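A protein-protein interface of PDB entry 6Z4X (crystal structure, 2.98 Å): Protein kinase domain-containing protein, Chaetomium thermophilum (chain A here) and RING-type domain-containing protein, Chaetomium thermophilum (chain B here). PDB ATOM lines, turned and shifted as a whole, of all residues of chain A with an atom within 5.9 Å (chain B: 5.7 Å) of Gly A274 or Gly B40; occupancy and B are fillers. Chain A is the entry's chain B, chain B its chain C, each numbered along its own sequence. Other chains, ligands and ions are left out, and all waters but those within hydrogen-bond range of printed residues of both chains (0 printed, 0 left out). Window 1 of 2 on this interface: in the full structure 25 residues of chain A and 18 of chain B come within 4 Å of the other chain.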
ATOM      1  N   HIS A 212     -10.320  19.204  10.670  1.00  0.00           N
ATOM      2  CA  HIS A 212     -11.331  18.178  10.919  1.00  0.00           C
ATOM      3  C   HIS A 212     -12.694  18.572  10.362  1.00  0.00           C
ATOM      4  O   HIS A 212     -13.456  17.704   9.920  1.00  0.00           O
ATOM      5  CB  HIS A 212     -11.425  17.888  12.418  1.00  0.00           C
ATOM      6  CG  HIS A 212     -10.197  17.248  12.989  1.00  0.00           C
ATOM      7  ND1 HIS A 212     -10.053  16.985  14.334  1.00  0.00           N
ATOM      8  CD2 HIS A 212      -9.063  16.804  12.396  1.00  0.00           C
ATOM      9  CE1 HIS A 212      -8.878  16.419  14.547  1.00  0.00           C
ATOM     10  NE2 HIS A 212      -8.258  16.296  13.387  1.00  0.00           N
ATOM     11  N   LEU A 217      -7.315  14.433   8.469  1.00  0.00           N
ATOM     12  CA  LEU A 217      -6.436  14.191   9.603  1.00  0.00           C
ATOM     13  C   LEU A 217      -5.030  14.639   9.234  1.00  0.00           C
ATOM     14  O   LEU A 217      -4.546  14.335   8.139  1.00  0.00           O
ATOM     15  CB  LEU A 217      -6.442  12.712   9.989  1.00  0.00           C
ATOM     16  CG  LEU A 217      -7.786  12.141  10.438  1.00  0.00           C
ATOM     17  CD1 LEU A 217      -7.697  10.636  10.605  1.00  0.00           C
ATOM     18  CD2 LEU A 217      -8.227  12.795  11.737  1.00  0.00           C
ATOM     19  N   PHE A 245     -10.801  11.437   6.237  1.00  0.00           N
ATOM     20  CA  PHE A 245     -11.505  10.575   7.178  1.00  0.00           C
ATOM     21  C   PHE A 245     -11.918   9.280   6.487  1.00  0.00           C
ATOM     22  O   PHE A 245     -12.646   9.303   5.488  1.00  0.00           O
ATOM     23  CB  PHE A 245     -12.728  11.296   7.743  1.00  0.00           C
ATOM     24  CG  PHE A 245     -12.398  12.397   8.716  1.00  0.00           C
ATOM     25  CD1 PHE A 245     -11.085  12.790   8.932  1.00  0.00           C
ATOM     26  CD2 PHE A 245     -13.406  13.039   9.418  1.00  0.00           C
ATOM     27  CE1 PHE A 245     -10.789  13.809   9.824  1.00  0.00           C
ATOM     28  CE2 PHE A 245     -13.116  14.054  10.313  1.00  0.00           C
ATOM     29  CZ  PHE A 245     -11.807  14.439  10.516  1.00  0.00           C
ATOM     30  N   GLU A 265      -3.424   4.957  21.102  1.00  0.00           N
ATOM     31  CA  GLU A 265      -4.078   4.005  20.209  1.00  0.00           C
ATOM     32  C   GLU A 265      -3.243   3.729  18.963  1.00  0.00           C
ATOM     33  O   GLU A 265      -3.292   2.619  18.421  1.00  0.00           O
ATOM     34  CB  GLU A 265      -5.479   4.496  19.827  1.00  0.00           C
ATOM     35  CG  GLU A 265      -5.533   5.785  19.020  1.00  0.00           C
ATOM     36  CD  GLU A 265      -5.746   7.011  19.889  1.00  0.00           C
ATOM     37  OE1 GLU A 265      -5.168   7.075  20.995  1.00  0.00           O
ATOM     38  OE2 GLU A 265      -6.509   7.907  19.473  1.00  0.00           O
ATOM     39  N   HIS A 272      -8.456   1.788  12.952  1.00  0.00           N
ATOM     40  CA  HIS A 272      -9.713   2.505  12.745  1.00  0.00           C
ATOM     41  C   HIS A 272      -9.816   3.553  13.848  1.00  0.00           C
ATOM     42  O   HIS A 272     -10.417   3.311  14.899  1.00  0.00           O
ATOM     43  CB  HIS A 272     -10.903   1.547  12.752  1.00  0.00           C
ATOM     44  CG  HIS A 272     -10.798   0.444  11.743  1.00  0.00           C
ATOM     45  ND1 HIS A 272     -11.282   0.561  10.458  1.00  0.00           N
ATOM     46  CD2 HIS A 272     -10.264  -0.798  11.833  1.00  0.00           C
ATOM     47  CE1 HIS A 272     -11.053  -0.562   9.800  1.00  0.00           C
ATOM     48  NE2 HIS A 272     -10.436  -1.402  10.611  1.00  0.00           N
ATOM     49  N   TYR A 273      -9.226   4.718  13.610  1.00  0.00           N
ATOM     50  CA  TYR A 273      -9.227   5.813  14.569  1.00  0.00           C
ATOM     51  C   TYR A 273      -9.899   7.039  13.956  1.00  0.00           C
ATOM     52  O   TYR A 273     -10.417   7.001  12.837  1.00  0.00           O
ATOM     53  CB  TYR A 273      -7.802   6.132  15.034  1.00  0.00           C
ATOM     54  CG  TYR A 273      -6.782   6.228  13.919  1.00  0.00           C
ATOM     55  CD1 TYR A 273      -6.642   7.392  13.175  1.00  0.00           C
ATOM     56  CD2 TYR A 273      -5.940   5.159  13.627  1.00  0.00           C
ATOM     57  CE1 TYR A 273      -5.705   7.484  12.160  1.00  0.00           C
ATOM     58  CE2 TYR A 273      -4.998   5.244  12.616  1.00  0.00           C
ATOM     59  CZ  TYR A 273      -4.886   6.409  11.886  1.00  0.00           C
ATOM     60  OH  TYR A 273      -3.954   6.496  10.877  1.00  0.00           O
ATOM     61  N   GLY A 274      -9.885   8.138  14.706  1.00  0.00           N
ATOM     62  CA  GLY A 274     -10.516   9.361  14.252  1.00  0.00           C
ATOM     63  C   GLY A 274      -9.726  10.613  14.567  1.00  0.00           C
ATOM     64  O   GLY A 274      -8.513  10.554  14.793  1.00  0.00           O
ATOM     65  N   GLY A 275     -10.410  11.756  14.598  1.00  0.00           N
ATOM     66  CA  GLY A 275      -9.738  13.020  14.838  1.00  0.00           C
ATOM     67  C   GLY A 275      -9.013  13.099  16.165  1.00  0.00           C
ATOM     68  O   GLY A 275      -8.114  13.933  16.319  1.00  0.00           O
ATOM     69  N   ALA A 276      -9.382  12.253  17.131  1.00  0.00           N
ATOM     70  CA  ALA A 276      -8.737  12.300  18.438  1.00  0.00           C
ATOM     71  C   ALA A 276      -7.227  12.164  18.322  1.00  0.00           C
ATOM     72  O   ALA A 276      -6.486  12.794  19.087  1.00  0.00           O
ATOM     73  CB  ALA A 276      -9.299  11.201  19.342  1.00  0.00           C
ATOM     74  N   VAL A 277      -6.751  11.377  17.352  1.00  0.00           N
ATOM     75  CA  VAL A 277      -5.313  11.181  17.190  1.00  0.00           C
ATOM     76  C   VAL A 277      -4.609  12.522  17.049  1.00  0.00           C
ATOM     77  O   VAL A 277      -3.508  12.721  17.578  1.00  0.00           O
ATOM     78  CB  VAL A 277      -5.027  10.270  15.981  1.00  0.00           C
ATOM     79  CG1 VAL A 277      -5.622   8.892  16.197  1.00  0.00           C
ATOM     80  CG2 VAL A 277      -5.557  10.906  14.701  1.00  0.00           C
ATOM     81  N   ASP A 278      -5.242  13.471  16.355  1.00  0.00           N
ATOM     82  CA  ASP A 278      -4.643  14.794  16.214  1.00  0.00           C
ATOM     83  C   ASP A 278      -4.684  15.556  17.531  1.00  0.00           C
ATOM     84  O   ASP A 278      -3.682  16.161  17.934  1.00  0.00           O
ATOM     85  CB  ASP A 278      -5.358  15.581  15.115  1.00  0.00           C
ATOM     86  CG  ASP A 278      -4.885  15.204  13.718  1.00  0.00           C
ATOM     87  OD1 ASP A 278      -3.693  14.858  13.559  1.00  0.00           O
ATOM     88  OD2 ASP A 278      -5.708  15.257  12.778  1.00  0.00           O
ATOM     89  N   ASP A 367      -8.268   6.883  26.545  1.00  0.00           N
ATOM     90  CA  ASP A 367      -9.300   6.429  25.623  1.00  0.00           C
ATOM     91  C   ASP A 367      -9.625   7.550  24.642  1.00  0.00           C
ATOM     92  O   ASP A 367     -10.124   8.602  25.063  1.00  0.00           O
ATOM     93  CB  ASP A 367     -10.546   6.003  26.396  1.00  0.00           C
ATOM     94  CG  ASP A 367     -11.581   5.334  25.512  1.00  0.00           C
ATOM     95  OD1 ASP A 367     -11.451   5.409  24.274  1.00  0.00           O
ATOM     96  OD2 ASP A 367     -12.522   4.723  26.058  1.00  0.00           O
ATOM     97  N   PRO A 368      -9.355   7.384  23.346  1.00  0.00           N
ATOM     98  CA  PRO A 368      -9.689   8.452  22.389  1.00  0.00           C
ATOM     99  C   PRO A 368     -11.168   8.783  22.352  1.00  0.00           C
ATOM    100  O   PRO A 368     -11.536   9.881  21.915  1.00  0.00           O
ATOM    101  CB  PRO A 368      -9.206   7.886  21.045  1.00  0.00           C
ATOM    102  CG  PRO A 368      -9.159   6.408  21.246  1.00  0.00           C
ATOM    103  CD  PRO A 368      -8.783   6.202  22.683  1.00  0.00           C
ATOM    104  N   LYS A 369     -12.028   7.866  22.795  1.00  0.00           N
ATOM    105  CA  LYS A 369     -13.457   8.147  22.833  1.00  0.00           C
ATOM    106  C   LYS A 369     -13.790   9.244  23.839  1.00  0.00           C
ATOM    107  O   LYS A 369     -14.738  10.008  23.626  1.00  0.00           O
ATOM    108  CB  LYS A 369     -14.224   6.864  23.154  1.00  0.00           C
ATOM    109  CG  LYS A 369     -14.048   5.776  22.104  1.00  0.00           C
ATOM    110  CD  LYS A 369     -14.762   4.495  22.482  1.00  0.00           C
ATOM    111  CE  LYS A 369     -14.037   3.762  23.595  1.00  0.00           C
ATOM    112  NZ  LYS A 369     -14.805   2.561  24.051  1.00  0.00           N
ATOM    113  N   GLN B  35     -12.433  -3.274  17.263  1.00  0.00           N
ATOM    114  CA  GLN B  35     -11.396  -2.351  16.817  1.00  0.00           C
ATOM    115  C   GLN B  35     -11.945  -0.944  16.614  1.00  0.00           C
ATOM    116  O   GLN B  35     -11.273   0.038  16.943  1.00  0.00           O
ATOM    117  CB  GLN B  35     -10.750  -2.865  15.533  1.00  0.00           C
ATOM    118  CG  GLN B  35     -10.102  -4.230  15.686  1.00  0.00           C
ATOM    119  CD  GLN B  35      -9.000  -4.235  16.728  1.00  0.00           C
ATOM    120  OE1 GLN B  35      -8.386  -3.205  17.000  1.00  0.00           O
ATOM    121  NE2 GLN B  35      -8.750  -5.397  17.322  1.00  0.00           N
ATOM    122  N   HIS B  36     -13.172  -0.822  16.099  1.00  0.00           N
ATOM    123  CA  HIS B  36     -13.715   0.504  15.813  1.00  0.00           C
ATOM    124  C   HIS B  36     -14.046   1.269  17.089  1.00  0.00           C
ATOM    125  O   HIS B  36     -13.785   2.475  17.178  1.00  0.00           O
ATOM    126  CB  HIS B  36     -14.944   0.390  14.913  1.00  0.00           C
ATOM    127  CG  HIS B  36     -14.611   0.134  13.477  1.00  0.00           C
ATOM    128  ND1 HIS B  36     -14.028  -1.037  13.043  1.00  0.00           N
ATOM    129  CD2 HIS B  36     -14.768   0.906  12.375  1.00  0.00           C
ATOM    130  CE1 HIS B  36     -13.849  -0.980  11.735  1.00  0.00           C
ATOM    131  NE2 HIS B  36     -14.288   0.190  11.305  1.00  0.00           N
ATOM    132  N   ILE B  37     -14.621   0.597  18.086  1.00  0.00           N
ATOM    133  CA  ILE B  37     -14.946   1.286  19.330  1.00  0.00           C
ATOM    134  C   ILE B  37     -13.679   1.567  20.128  1.00  0.00           C
ATOM    135  O   ILE B  37     -13.432   2.703  20.549  1.00  0.00           O
ATOM    136  CB  ILE B  37     -15.969   0.483  20.154  1.00  0.00           C
ATOM    137  CG1 ILE B  37     -15.481  -0.946  20.389  1.00  0.00           C
ATOM    138  CG2 ILE B  37     -17.326   0.482  19.465  1.00  0.00           C
ATOM    139  CD1 ILE B  37     -16.546  -1.861  20.958  1.00  0.00           C
ATOM    140  N   THR B  38     -12.854   0.540  20.350  1.00  0.00           N
ATOM    141  CA  THR B  38     -11.670   0.716  21.185  1.00  0.00           C
ATOM    142  C   THR B  38     -10.597   1.569  20.512  1.00  0.00           C
ATOM    143  O   THR B  38      -9.718   2.092  21.205  1.00  0.00           O
ATOM    144  CB  THR B  38     -11.093  -0.646  21.577  1.00  0.00           C
ATOM    145  OG1 THR B  38     -10.326  -0.507  22.779  1.00  0.00           O
ATOM    146  CG2 THR B  38     -10.198  -1.185  20.470  1.00  0.00           C
ATOM    147  N   GLY B  39     -10.646   1.726  19.187  1.00  0.00           N
ATOM    148  CA  GLY B  39      -9.677   2.536  18.476  1.00  0.00           C
ATOM    149  C   GLY B  39     -10.054   3.983  18.269  1.00  0.00           C
ATOM    150  O   GLY B  39      -9.234   4.759  17.770  1.00  0.00           O
ATOM    151  N   GLY B  40     -11.278   4.366  18.625  1.00  0.00           N
ATOM    152  CA  GLY B  40     -11.686   5.754  18.560  1.00  0.00           C
ATOM    153  C   GLY B  40     -12.236   6.218  17.232  1.00  0.00           C
ATOM    154  O   GLY B  40     -12.126   7.408  16.912  1.00  0.00           O
ATOM    155  N   TYR B  41     -12.824   5.321  16.442  1.00  0.00           N
ATOM    156  CA  TYR B  41     -13.431   5.724  15.181  1.00  0.00           C
ATOM    157  C   TYR B  41     -14.727   6.478  15.452  1.00  0.00           C
ATOM    158  O   TYR B  41     -15.555   6.043  16.258  1.00  0.00           O
ATOM    159  CB  TYR B  41     -13.696   4.502  14.303  1.00  0.00           C
ATOM    160  CG  TYR B  41     -14.269   4.843  12.946  1.00  0.00           C
ATOM    161  CD1 TYR B  41     -15.633   5.027  12.774  1.00  0.00           C
ATOM    162  CD2 TYR B  41     -13.445   4.979  11.837  1.00  0.00           C
ATOM    163  CE1 TYR B  41     -16.161   5.342  11.538  1.00  0.00           C
ATOM    164  CE2 TYR B  41     -13.964   5.293  10.596  1.00  0.00           C
ATOM    165  CZ  TYR B  41     -15.322   5.472  10.453  1.00  0.00           C
ATOM    166  OH  TYR B  41     -15.840   5.784   9.219  1.00  0.00           O
ATOM    167  N   SER B  42     -14.905   7.610  14.774  1.00  0.00           N
ATOM    168  CA  SER B  42     -16.055   8.486  14.985  1.00  0.00           C
ATOM    169  C   SER B  42     -17.115   8.216  13.923  1.00  0.00           C
ATOM    170  O   SER B  42     -16.951   8.599  12.760  1.00  0.00           O
ATOM    171  CB  SER B  42     -15.630   9.951  14.958  1.00  0.00           C
ATOM    172  OG  SER B  42     -16.760  10.806  15.003  1.00  0.00           O
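The backbone NH of Gly A274 is in hydrogen-bond range of the backbone carbonyl oxygen of Gly B40 (3.2 Å).
O of Gly B39 sits close to O of His A272.
O of His A272 sits at hydrogen-bond distance from N of Tyr B41 (3.5 Å).
A ring nitrogen (ND1) of His A272 is in hydrogen-bond range of a ring nitrogen (NE2) of His B36 (3.1 Å).
O of His B36 is in hydrogen-bond range of N of Tyr B41 (3.1 Å).
The side-chain amino group (NZ) of Lys A369 is in salt-bridge range of the side-chain carboxylate (OD2) of Asp A367, at 3.7 Å.
His A272 touches Gln B35.
Gly B40 touches His A272.
Gly B39 touches Tyr A273 (O to CA, 3.4 Å).
O of Gly B40 touches C of Tyr A273, 3.7 Å away.
Tyr B41 touches Tyr A273.
Pro A368 touches Gly B39 (CG to O, 3.8 Å).
Pro A368 touches Gly B40.
Ile B37 touches Lys A369.
Of the printed residues of chain B, His A272 touches Gln B35 (3.95 Å), His B36 (3.1 Å), Gly B39 (3.4 Å), Gly B40 (3.97 Å) and Tyr B41 (3.5 Å).
Gly A274 touches one residue of chain B.
Printed residues of chain B within 4 Å of Pro A368: Gly B39 and Gly B40.
Of the printed residues of chain B, Lys A369 touches Ile B37.
Printed residues of chain A within 4 Å of Gln B35: His A272 (3.95 Å).
Printed residues of chain A within 4 Å of Gly B39: His A272 (3.4 Å), Tyr A273 (3.4 Å) and Pro A368 (3.8 Å).
Of chain A, only His A272, Tyr A273, Gly A274 and Pro A368 come within 4 Å of Gly B40.
The nearest residue of chain A that does not touch Gly B40 is Lys A369 (4.3 Å).
Along chain A the printed residues that touch a printed residue of chain B span positions 272 to 369.
Among the printed residues, no Asp or Glu carboxylate lies within 4 Å of a Lys or Arg side-chain nitrogen of the other chain.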
